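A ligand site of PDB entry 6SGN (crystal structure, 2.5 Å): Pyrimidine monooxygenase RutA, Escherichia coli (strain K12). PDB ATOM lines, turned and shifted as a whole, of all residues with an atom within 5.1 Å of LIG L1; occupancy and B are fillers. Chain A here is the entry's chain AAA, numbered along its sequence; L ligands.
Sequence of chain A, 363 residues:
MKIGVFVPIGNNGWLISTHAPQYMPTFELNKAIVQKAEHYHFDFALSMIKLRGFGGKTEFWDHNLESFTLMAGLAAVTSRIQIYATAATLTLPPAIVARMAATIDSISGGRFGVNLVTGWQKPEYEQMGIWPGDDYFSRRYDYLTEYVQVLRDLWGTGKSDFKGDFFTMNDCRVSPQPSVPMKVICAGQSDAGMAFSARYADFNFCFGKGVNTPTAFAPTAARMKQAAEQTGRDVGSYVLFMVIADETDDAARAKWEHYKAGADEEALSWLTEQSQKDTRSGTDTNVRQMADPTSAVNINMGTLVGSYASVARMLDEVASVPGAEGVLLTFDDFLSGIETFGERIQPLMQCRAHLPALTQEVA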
ATOM      1  N   PHE A   6      -7.493 -32.686  18.425  1.00  0.00           N
ATOM      2  CA  PHE A   6      -8.791 -32.089  18.272  1.00  0.00           C
ATOM      3  C   PHE A   6      -9.138 -32.108  16.787  1.00  0.00           C
ATOM      4  O   PHE A   6      -8.757 -31.195  16.054  1.00  0.00           O
ATOM      5  CB  PHE A   6      -8.718 -30.679  18.867  1.00  0.00           C
ATOM      6  CG  PHE A   6      -9.996 -30.096  19.384  1.00  0.00           C
ATOM      7  CD1 PHE A   6     -11.087 -30.895  19.672  1.00  0.00           C
ATOM      8  CD2 PHE A   6     -10.101 -28.736  19.620  1.00  0.00           C
ATOM      9  CE1 PHE A   6     -12.259 -30.340  20.151  1.00  0.00           C
ATOM     10  CE2 PHE A   6     -11.259 -28.192  20.137  1.00  0.00           C
ATOM     11  CZ  PHE A   6     -12.349 -28.990  20.379  1.00  0.00           C
ATOM     12  N   LEU A  46     -10.640 -36.202  19.905  1.00  0.00           N
ATOM     13  CA  LEU A  46     -11.876 -35.565  20.315  1.00  0.00           C
ATOM     14  C   LEU A  46     -12.417 -34.685  19.183  1.00  0.00           C
ATOM     15  O   LEU A  46     -11.693 -33.918  18.540  1.00  0.00           O
ATOM     16  CB  LEU A  46     -11.595 -34.735  21.558  1.00  0.00           C
ATOM     17  CG  LEU A  46     -12.662 -33.709  21.934  1.00  0.00           C
ATOM     18  CD1 LEU A  46     -13.955 -34.418  22.325  1.00  0.00           C
ATOM     19  CD2 LEU A  46     -12.145 -32.838  23.046  1.00  0.00           C
ATOM     20  N   MET A  48     -15.318 -31.789  18.692  1.00  0.00           N
ATOM     21  CA  MET A  48     -16.415 -30.917  19.108  1.00  0.00           C
ATOM     22  C   MET A  48     -17.713 -31.220  18.342  1.00  0.00           C
ATOM     23  O   MET A  48     -17.805 -32.176  17.569  1.00  0.00           O
ATOM     24  CB  MET A  48     -16.058 -29.449  18.875  1.00  0.00           C
ATOM     25  CG  MET A  48     -15.882 -29.095  17.399  1.00  0.00           C
ATOM     26  SD  MET A  48     -15.472 -27.308  17.154  1.00  0.00           S
ATOM     27  CE  MET A  48     -16.832 -26.617  18.094  1.00  0.00           C
ATOM     28  N   ILE A  49     -18.728 -30.390  18.625  1.00  0.00           N
ATOM     29  CA  ILE A  49     -19.930 -30.252  17.823  1.00  0.00           C
ATOM     30  C   ILE A  49     -20.156 -28.765  17.610  1.00  0.00           C
ATOM     31  O   ILE A  49     -19.962 -27.970  18.540  1.00  0.00           O
ATOM     32  CB  ILE A  49     -21.146 -30.911  18.513  1.00  0.00           C
ATOM     33  CG1 ILE A  49     -22.319 -31.161  17.553  1.00  0.00           C
ATOM     34  CG2 ILE A  49     -21.577 -30.090  19.706  1.00  0.00           C
ATOM     35  CD1 ILE A  49     -22.168 -32.361  16.654  1.00  0.00           C
ATOM     36  N   THR A  86     -18.808 -35.449  21.231  1.00  0.00           N
ATOM     37  CA  THR A  86     -19.366 -34.420  22.078  1.00  0.00           C
ATOM     38  C   THR A  86     -20.867 -34.457  21.916  1.00  0.00           C
ATOM     39  O   THR A  86     -21.320 -34.454  20.800  1.00  0.00           O
ATOM     40  CB  THR A  86     -18.865 -33.046  21.626  1.00  0.00           C
ATOM     41  OG1 THR A  86     -17.473 -33.071  21.928  1.00  0.00           O
ATOM     42  CG2 THR A  86     -19.550 -31.912  22.338  1.00  0.00           C
ATOM     43  N   ASN A 115     -18.162 -36.377  25.749  1.00  0.00           N
ATOM     44  CA  ASN A 115     -17.715 -35.100  26.238  1.00  0.00           C
ATOM     45  C   ASN A 115     -18.990 -34.291  26.334  1.00  0.00           C
ATOM     46  O   ASN A 115     -19.593 -34.028  25.298  1.00  0.00           O
ATOM     47  CB  ASN A 115     -16.722 -34.428  25.291  1.00  0.00           C
ATOM     48  CG  ASN A 115     -16.503 -32.956  25.645  1.00  0.00           C
ATOM     49  OD1 ASN A 115     -16.470 -32.569  26.806  1.00  0.00           O
ATOM     50  ND2 ASN A 115     -16.433 -32.099  24.636  1.00  0.00           N
ATOM     51  N   VAL A 117     -21.489 -31.233  27.093  1.00  0.00           N
ATOM     52  CA  VAL A 117     -21.432 -29.819  26.757  1.00  0.00           C
ATOM     53  C   VAL A 117     -22.818 -29.207  26.990  1.00  0.00           C
ATOM     54  O   VAL A 117     -23.847 -29.794  26.627  1.00  0.00           O
ATOM     55  CB  VAL A 117     -20.886 -29.635  25.330  1.00  0.00           C
ATOM     56  CG1 VAL A 117     -21.671 -28.666  24.459  1.00  0.00           C
ATOM     57  CG2 VAL A 117     -19.386 -29.312  25.312  1.00  0.00           C
ATOM     58  N   THR A 118     -22.805 -28.038  27.629  1.00  0.00           N
ATOM     59  CA  THR A 118     -24.007 -27.283  27.935  1.00  0.00           C
ATOM     60  C   THR A 118     -24.606 -26.740  26.644  1.00  0.00           C
ATOM     61  O   THR A 118     -25.814 -26.792  26.446  1.00  0.00           O
ATOM     62  CB  THR A 118     -23.732 -26.117  28.909  1.00  0.00           C
ATOM     63  OG1 THR A 118     -22.713 -25.244  28.434  1.00  0.00           O
ATOM     64  CG2 THR A 118     -23.386 -26.620  30.298  1.00  0.00           C
ATOM     65  N   GLY A 119     -23.732 -26.233  25.760  1.00  0.00           N
ATOM     66  CA  GLY A 119     -24.083 -25.290  24.714  1.00  0.00           C
ATOM     67  C   GLY A 119     -23.983 -23.870  25.250  1.00  0.00           C
ATOM     68  O   GLY A 119     -24.484 -23.601  26.334  1.00  0.00           O
ATOM     69  N   TRP A 120     -23.312 -22.969  24.518  1.00  0.00           N
ATOM     70  CA  TRP A 120     -23.103 -21.628  25.035  1.00  0.00           C
ATOM     71  C   TRP A 120     -23.798 -20.566  24.183  1.00  0.00           C
ATOM     72  O   TRP A 120     -24.459 -19.691  24.739  1.00  0.00           O
ATOM     73  CB  TRP A 120     -21.606 -21.328  25.293  1.00  0.00           C
ATOM     74  CG  TRP A 120     -20.764 -21.212  24.055  1.00  0.00           C
ATOM     75  CD1 TRP A 120     -20.655 -22.130  23.052  1.00  0.00           C
ATOM     76  CD2 TRP A 120     -19.882 -20.123  23.715  1.00  0.00           C
ATOM     77  NE1 TRP A 120     -19.790 -21.673  22.096  1.00  0.00           N
ATOM     78  CE2 TRP A 120     -19.292 -20.459  22.471  1.00  0.00           C
ATOM     79  CE3 TRP A 120     -19.533 -18.909  24.318  1.00  0.00           C
ATOM     80  CZ2 TRP A 120     -18.377 -19.615  21.830  1.00  0.00           C
ATOM     81  CZ3 TRP A 120     -18.631 -18.071  23.688  1.00  0.00           C
ATOM     82  CH2 TRP A 120     -18.058 -18.426  22.461  1.00  0.00           C
ATOM     83  N   GLU A 124     -27.104 -21.398  17.943  1.00  0.00           N
ATOM     84  CA  GLU A 124     -27.028 -22.822  17.644  1.00  0.00           C
ATOM     85  C   GLU A 124     -28.385 -23.509  17.898  1.00  0.00           C
ATOM     86  O   GLU A 124     -28.774 -24.394  17.134  1.00  0.00           O
ATOM     87  CB  GLU A 124     -25.887 -23.496  18.424  1.00  0.00           C
ATOM     88  CG  GLU A 124     -24.494 -23.223  17.870  1.00  0.00           C
ATOM     89  CD  GLU A 124     -23.337 -23.966  18.529  1.00  0.00           C
ATOM     90  OE1 GLU A 124     -23.294 -25.234  18.425  1.00  0.00           O
ATOM     91  OE2 GLU A 124     -22.487 -23.297  19.159  1.00  0.00           O
ATOM     92  N   TYR A 125     -29.104 -23.068  18.936  1.00  0.00           N
ATOM     93  CA  TYR A 125     -30.252 -23.784  19.489  1.00  0.00           C
ATOM     94  C   TYR A 125     -31.556 -23.073  19.144  1.00  0.00           C
ATOM     95  O   TYR A 125     -32.598 -23.715  19.055  1.00  0.00           O
ATOM     96  CB  TYR A 125     -30.102 -24.024  20.992  1.00  0.00           C
ATOM     97  CG  TYR A 125     -28.802 -24.713  21.326  1.00  0.00           C
ATOM     98  CD1 TYR A 125     -28.665 -26.084  21.158  1.00  0.00           C
ATOM     99  CD2 TYR A 125     -27.695 -23.986  21.725  1.00  0.00           C
ATOM    100  CE1 TYR A 125     -27.470 -26.730  21.399  1.00  0.00           C
ATOM    101  CE2 TYR A 125     -26.486 -24.622  21.979  1.00  0.00           C
ATOM    102  CZ  TYR A 125     -26.376 -25.990  21.831  1.00  0.00           C
ATOM    103  OH  TYR A 125     -25.176 -26.616  22.081  1.00  0.00           O
ATOM    104  N   ARG A 140     -27.887 -24.271  33.368  1.00  0.00           N
ATOM    105  CA  ARG A 140     -27.395 -25.347  32.510  1.00  0.00           C
ATOM    106  C   ARG A 140     -26.819 -26.501  33.337  1.00  0.00           C
ATOM    107  O   ARG A 140     -27.090 -27.669  33.041  1.00  0.00           O
ATOM    108  CB  ARG A 140     -26.376 -24.806  31.509  1.00  0.00           C
ATOM    109  CG  ARG A 140     -25.298 -23.910  32.098  1.00  0.00           C
ATOM    110  CD  ARG A 140     -24.785 -22.995  31.014  1.00  0.00           C
ATOM    111  NE  ARG A 140     -23.756 -22.115  31.535  1.00  0.00           N
ATOM    112  CZ  ARG A 140     -22.473 -22.145  31.176  1.00  0.00           C
ATOM    113  NH1 ARG A 140     -21.607 -21.311  31.730  1.00  0.00           N
ATOM    114  NH2 ARG A 140     -22.056 -23.010  30.263  1.00  0.00           N
ATOM    115  N   TYR A 141     -26.033 -26.152  34.375  1.00  0.00           N
ATOM    116  CA  TYR A 141     -25.411 -27.108  35.275  1.00  0.00           C
ATOM    117  C   TYR A 141     -26.436 -27.863  36.104  1.00  0.00           C
ATOM    118  O   TYR A 141     -26.252 -29.036  36.403  1.00  0.00           O
ATOM    119  CB  TYR A 141     -24.220 -26.469  35.990  1.00  0.00           C
ATOM    120  CG  TYR A 141     -23.065 -26.272  35.029  1.00  0.00           C
ATOM    121  CD1 TYR A 141     -22.390 -27.366  34.504  1.00  0.00           C
ATOM    122  CD2 TYR A 141     -22.698 -25.014  34.578  1.00  0.00           C
ATOM    123  CE1 TYR A 141     -21.364 -27.233  33.583  1.00  0.00           C
ATOM    124  CE2 TYR A 141     -21.661 -24.855  33.668  1.00  0.00           C
ATOM    125  CZ  TYR A 141     -20.995 -25.971  33.155  1.00  0.00           C
ATOM    126  OH  TYR A 141     -19.985 -25.869  32.244  1.00  0.00           O
ATOM    127  N   ALA A 187     -15.829 -29.540  29.829  1.00  0.00           N
ATOM    128  CA  ALA A 187     -14.957 -28.429  29.491  1.00  0.00           C
ATOM    129  C   ALA A 187     -15.505 -27.121  30.070  1.00  0.00           C
ATOM    130  O   ALA A 187     -15.448 -26.086  29.426  1.00  0.00           O
ATOM    131  CB  ALA A 187     -14.806 -28.363  27.991  1.00  0.00           C
ATOM    132  N   GLY A 188     -16.026 -27.175  31.296  1.00  0.00           N
ATOM    133  CA  GLY A 188     -16.417 -25.975  32.016  1.00  0.00           C
ATOM    134  C   GLY A 188     -15.235 -25.245  32.654  1.00  0.00           C
ATOM    135  O   GLY A 188     -14.332 -25.848  33.247  1.00  0.00           O
ATOM    136  N   GLN A 189     -15.266 -23.915  32.546  1.00  0.00           N
ATOM    137  CA  GLN A 189     -14.192 -23.078  33.035  1.00  0.00           C
ATOM    138  C   GLN A 189     -14.698 -22.320  34.245  1.00  0.00           C
ATOM    139  O   GLN A 189     -13.899 -21.863  35.061  1.00  0.00           O
ATOM    140  CB  GLN A 189     -13.742 -22.059  31.974  1.00  0.00           C
ATOM    141  CG  GLN A 189     -13.554 -22.601  30.566  1.00  0.00           C
ATOM    142  CD  GLN A 189     -12.474 -23.640  30.435  1.00  0.00           C
ATOM    143  OE1 GLN A 189     -11.287 -23.378  30.647  1.00  0.00           O
ATOM    144  NE2 GLN A 189     -12.880 -24.839  30.059  1.00  0.00           N
ATOM    145  N   SER A 190     -16.023 -22.148  34.343  1.00  0.00           N
ATOM    146  CA  SER A 190     -16.633 -21.479  35.481  1.00  0.00           C
ATOM    147  C   SER A 190     -16.630 -22.363  36.737  1.00  0.00           C
ATOM    148  O   SER A 190     -16.209 -23.526  36.714  1.00  0.00           O
ATOM    149  CB  SER A 190     -18.009 -20.988  35.114  1.00  0.00           C
ATOM    150  OG  SER A 190     -18.959 -22.045  35.140  1.00  0.00           O
ATOM    151  N   GLY A 193     -18.896 -25.060  36.494  1.00  0.00           N
ATOM    152  CA  GLY A 193     -18.414 -25.939  35.455  1.00  0.00           C
ATOM    153  C   GLY A 193     -17.459 -26.939  36.053  1.00  0.00           C
ATOM    154  O   GLY A 193     -17.605 -28.151  35.881  1.00  0.00           O
ATOM    155  N   PHE A 205     -11.356 -30.173  30.337  1.00  0.00           N
ATOM    156  CA  PHE A 205     -10.670 -29.508  29.244  1.00  0.00           C
ATOM    157  C   PHE A 205     -10.669 -28.023  29.489  1.00  0.00           C
ATOM    158  O   PHE A 205     -11.741 -27.450  29.657  1.00  0.00           O
ATOM    159  CB  PHE A 205     -11.312 -29.841  27.906  1.00  0.00           C
ATOM    160  CG  PHE A 205     -10.937 -31.229  27.448  1.00  0.00           C
ATOM    161  CD1 PHE A 205      -9.619 -31.657  27.502  1.00  0.00           C
ATOM    162  CD2 PHE A 205     -11.905 -32.130  27.029  1.00  0.00           C
ATOM    163  CE1 PHE A 205      -9.271 -32.939  27.129  1.00  0.00           C
ATOM    164  CE2 PHE A 205     -11.551 -33.413  26.643  1.00  0.00           C
ATOM    165  CZ  PHE A 205     -10.234 -33.828  26.705  1.00  0.00           C
ATOM    166  N   CYS A 206      -9.477 -27.427  29.522  1.00  0.00           N
ATOM    167  CA  CYS A 206      -9.419 -25.978  29.563  1.00  0.00           C
ATOM    168  C   CYS A 206      -8.575 -25.398  28.424  1.00  0.00           C
ATOM    169  O   CYS A 206      -7.867 -26.120  27.745  1.00  0.00           O
ATOM    170  CB  CYS A 206      -8.851 -25.459  30.878  1.00  0.00           C
ATOM    171  SG  CYS A 206      -7.171 -26.040  31.154  1.00  0.00           S
ATOM    172  N   PHE A 207      -8.602 -24.063  28.294  1.00  0.00           N
ATOM    173  CA  PHE A 207      -7.900 -23.401  27.208  1.00  0.00           C
ATOM    174  C   PHE A 207      -6.472 -23.071  27.636  1.00  0.00           C
ATOM    175  O   PHE A 207      -6.302 -22.479  28.694  1.00  0.00           O
ATOM    176  CB  PHE A 207      -8.632 -22.120  26.818  1.00  0.00           C
ATOM    177  CG  PHE A 207     -10.059 -22.333  26.371  1.00  0.00           C
ATOM    178  CD1 PHE A 207     -10.342 -22.898  25.132  1.00  0.00           C
ATOM    179  CD2 PHE A 207     -11.115 -21.992  27.208  1.00  0.00           C
ATOM    180  CE1 PHE A 207     -11.656 -23.094  24.740  1.00  0.00           C
ATOM    181  CE2 PHE A 207     -12.434 -22.207  26.806  1.00  0.00           C
ATOM    182  CZ  PHE A 207     -12.699 -22.750  25.575  1.00  0.00           C
ATOM    183  N   LEU A 240      -5.933 -27.107  25.853  1.00  0.00           N
ATOM    184  CA  LEU A 240      -5.967 -26.919  24.401  1.00  0.00           C
ATOM    185  C   LEU A 240      -4.936 -25.879  23.933  1.00  0.00           C
ATOM    186  O   LEU A 240      -4.932 -24.719  24.384  1.00  0.00           O
ATOM    187  CB  LEU A 240      -7.371 -26.506  24.010  1.00  0.00           C
ATOM    188  CG  LEU A 240      -7.540 -25.980  22.572  1.00  0.00           C
ATOM    189  CD1 LEU A 240      -7.537 -27.116  21.554  1.00  0.00           C
ATOM    190  CD2 LEU A 240      -8.826 -25.195  22.449  1.00  0.00           C
ATOM    191  N   LEU A 328      -4.504 -31.090  24.487  1.00  0.00           N
ATOM    192  CA  LEU A 328      -5.309 -31.279  23.319  1.00  0.00           C
ATOM    193  C   LEU A 328      -4.802 -30.330  22.232  1.00  0.00           C
ATOM    194  O   LEU A 328      -4.821 -29.109  22.409  1.00  0.00           O
ATOM    195  CB  LEU A 328      -6.750 -31.003  23.741  1.00  0.00           C
ATOM    196  CG  LEU A 328      -7.769 -31.115  22.626  1.00  0.00           C
ATOM    197  CD1 LEU A 328      -7.722 -32.485  22.004  1.00  0.00           C
ATOM    198  CD2 LEU A 328      -9.168 -30.746  23.146  1.00  0.00           C
HETATM  199  N1  LIG L   1     -18.726 -25.952  23.492  1.00  0.00           N
HETATM  200  C1  LIG L   1     -19.659 -26.511  22.638  1.00  0.00           C
HETATM  201  O1  LIG L   1     -20.805 -26.025  22.531  1.00  0.00           O
HETATM  202  N2  LIG L   1     -19.384 -27.593  21.880  1.00  0.00           N
HETATM  203  C2  LIG L   1     -18.173 -28.186  21.926  1.00  0.00           C
HETATM  204  O2  LIG L   1     -17.906 -29.191  21.246  1.00  0.00           O
HETATM  205  C3  LIG L   1     -17.116 -27.664  22.804  1.00  0.00           C
HETATM  206  N3  LIG L   1     -15.925 -28.266  22.849  1.00  0.00           N
HETATM  207  C4  LIG L   1     -14.959 -27.777  23.659  1.00  0.00           C
HETATM  208  C5  LIG L   1     -13.714 -28.412  23.698  1.00  0.00           C
HETATM  209  C6  LIG L   1     -12.691 -27.939  24.486  1.00  0.00           C
HETATM  210  C7  LIG L   1     -11.380 -28.662  24.487  1.00  0.00           C
HETATM  211  C8  LIG L   1     -12.853 -26.745  25.350  1.00  0.00           C
HETATM  212  C9  LIG L   1     -11.680 -26.294  26.210  1.00  0.00           C
HETATM  213  C10 LIG L   1     -14.105 -26.097  25.330  1.00  0.00           C
HETATM  214  C11 LIG L   1     -15.184 -26.552  24.517  1.00  0.00           C
HETATM  215  N4  LIG L   1     -16.474 -25.906  24.482  1.00  0.00           N
HETATM  216  C12 LIG L   1     -17.470 -26.468  23.639  1.00  0.00           C
HETATM  217  C13 LIG L   1     -16.790 -24.728  25.311  1.00  0.00           C
HETATM  218  C14 LIG L   1     -17.097 -25.202  26.751  1.00  0.00           C
HETATM  219  O3  LIG L   1     -18.003 -26.329  26.706  1.00  0.00           O
HETATM  220  C15 LIG L   1     -17.592 -24.117  27.754  1.00  0.00           C
HETATM  221  O4  LIG L   1     -18.814 -23.555  27.266  1.00  0.00           O
HETATM  222  C16 LIG L   1     -16.629 -22.941  28.114  1.00  0.00           C
HETATM  223  O5  LIG L   1     -15.241 -23.351  28.175  1.00  0.00           O
HETATM  224  C17 LIG L   1     -17.081 -22.063  29.319  1.00  0.00           C
HETATM  225  O6  LIG L   1     -17.263 -22.758  30.590  1.00  0.00           O
HETATM  226  P1  LIG L   1     -18.690 -22.863  31.393  1.00  0.00           P
HETATM  227  O7  LIG L   1     -19.142 -21.433  31.532  1.00  0.00           O
HETATM  228  O8  LIG L   1     -19.569 -23.689  30.487  1.00  0.00           O
HETATM  229  O9  LIG L   1     -18.402 -23.503  32.732  1.00  0.00           O
HETATM  230  O1  LG2 L   2     -12.871 -24.468  20.120  1.00  0.00           O
HETATM  231  O2  LG2 L   2     -17.509 -24.690  20.665  1.00  0.00           O
HETATM  232  N1  LG2 L   2     -15.191 -24.654  20.352  1.00  0.00           N
HETATM  233  N2  LG2 L   2     -16.296 -22.911  21.840  1.00  0.00           N
HETATM  234  C1  LG2 L   2     -14.013 -24.014  20.654  1.00  0.00           C
HETATM  235  C2  LG2 L   2     -13.898 -22.833  21.521  1.00  0.00           C
HETATM  236  C3  LG2 L   2     -16.316 -24.060  20.958  1.00  0.00           C
HETATM  237  C4  LG2 L   2     -15.074 -22.329  22.078  1.00  0.00           C
HETATM  238  C5  LG2 L   2     -11.752 -23.566  20.264  1.00  0.00           C
HETATM  239  C6  LG2 L   2     -18.714 -23.930  20.800  1.00  0.00           C
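NH2 of Arg 140 sits at hydrogen-bond distance from OG1 of Thr 118 (3.0 Å).
The backbone carbonyl oxygen (O) of Ala 187 lies within hydrogen-bond range of the side-chain amide nitrogen (NE2) of Gln 189 (2.9 Å).
O of Cys 206 lies within hydrogen-bond range of N of Leu 240 (2.9 Å).
The side-chain amide nitrogen (NE2) of Gln 189 is in hydrogen-bond range of the backbone carbonyl oxygen (O) of Phe 205 (2.9 Å).
The side-chain amide nitrogen (ND2) of Asn 115 sits at hydrogen-bond distance from the side-chain hydroxyl (OG1) of Thr 86.
The backbone NH (N) of Gly 193 is in hydrogen-bond range of the side-chain hydroxyl (OG) of Ser 190 (3.3 Å).
The side-chain hydroxyl (OG) of Ser 190 sits at hydrogen-bond distance from an oxygen (O9) of LIG L1, at 2.9 Å.
The guanidinium group (NH1) of Arg 140 is in salt-bridge range of an oxygen (O7) of LIG L1 (2.5 Å).
The backbone NH (N) of Ser 190 is in hydrogen-bond range of an oxygen (O9) of LIG L1 (3.2 Å).
N2 of LIG L1 sits at hydrogen-bond distance from O of Ile 49, 3.4 Å away.
N of Gln 189 is in hydrogen-bond range of O6 of LIG L1, 3.0 Å away.
O of Ala 187 is in hydrogen-bond range of O5 of LIG L1 (3.0 Å).
N of Ile 49 lies within hydrogen-bond range of O2 of LIG L1.
The side-chain amide nitrogen of Gln 189 lies close to an oxygen (O5) of LIG L1 (3.4 Å).
The side-chain hydroxyl (OH) of Tyr 141 sits at hydrogen-bond distance from an oxygen (O8) of LIG L1 (2.8 Å).
CZ of Phe 6 touches C5 of LIG L1, 3.6 Å away.
Met 48 touches LIG L1 (CB to O2, 3.0 Å).
Thr 86 touches LIG L1.
Val 117 touches LIG L1.
Trp 120 touches LIG L1 (CD1 to O1, 3.9 Å).
Gly 188 touches LIG L1 (CA to O9, 3.3 Å).
CA of Gly 193 touches O9 of LIG L1 (3.7 Å).
Phe 205 touches LIG L1 (CB to C7, 3.6 Å).
Cys 206 touches LIG L1.
Phe 207 touches LIG L1 (CE2 to O5, 3.3 Å).
Leu 328 touches LIG L1.
Hydrophobic or aromatic side chains that line LIG L1: Phe 6, Met 48, Ile 49, Val 117, Trp 120, Tyr 141, Ala 187, Phe 205, Phe 207 and Leu 328.
Within 4 Å of LIG L1: Phe 6, Met 48, Ile 49, Thr 86, Val 117, Trp 120, Arg 140, Tyr 141, Ala 187, Gly 188, Gln 189, Ser 190, Gly 193, Phe 205, Cys 206, Phe 207 and Leu 328.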
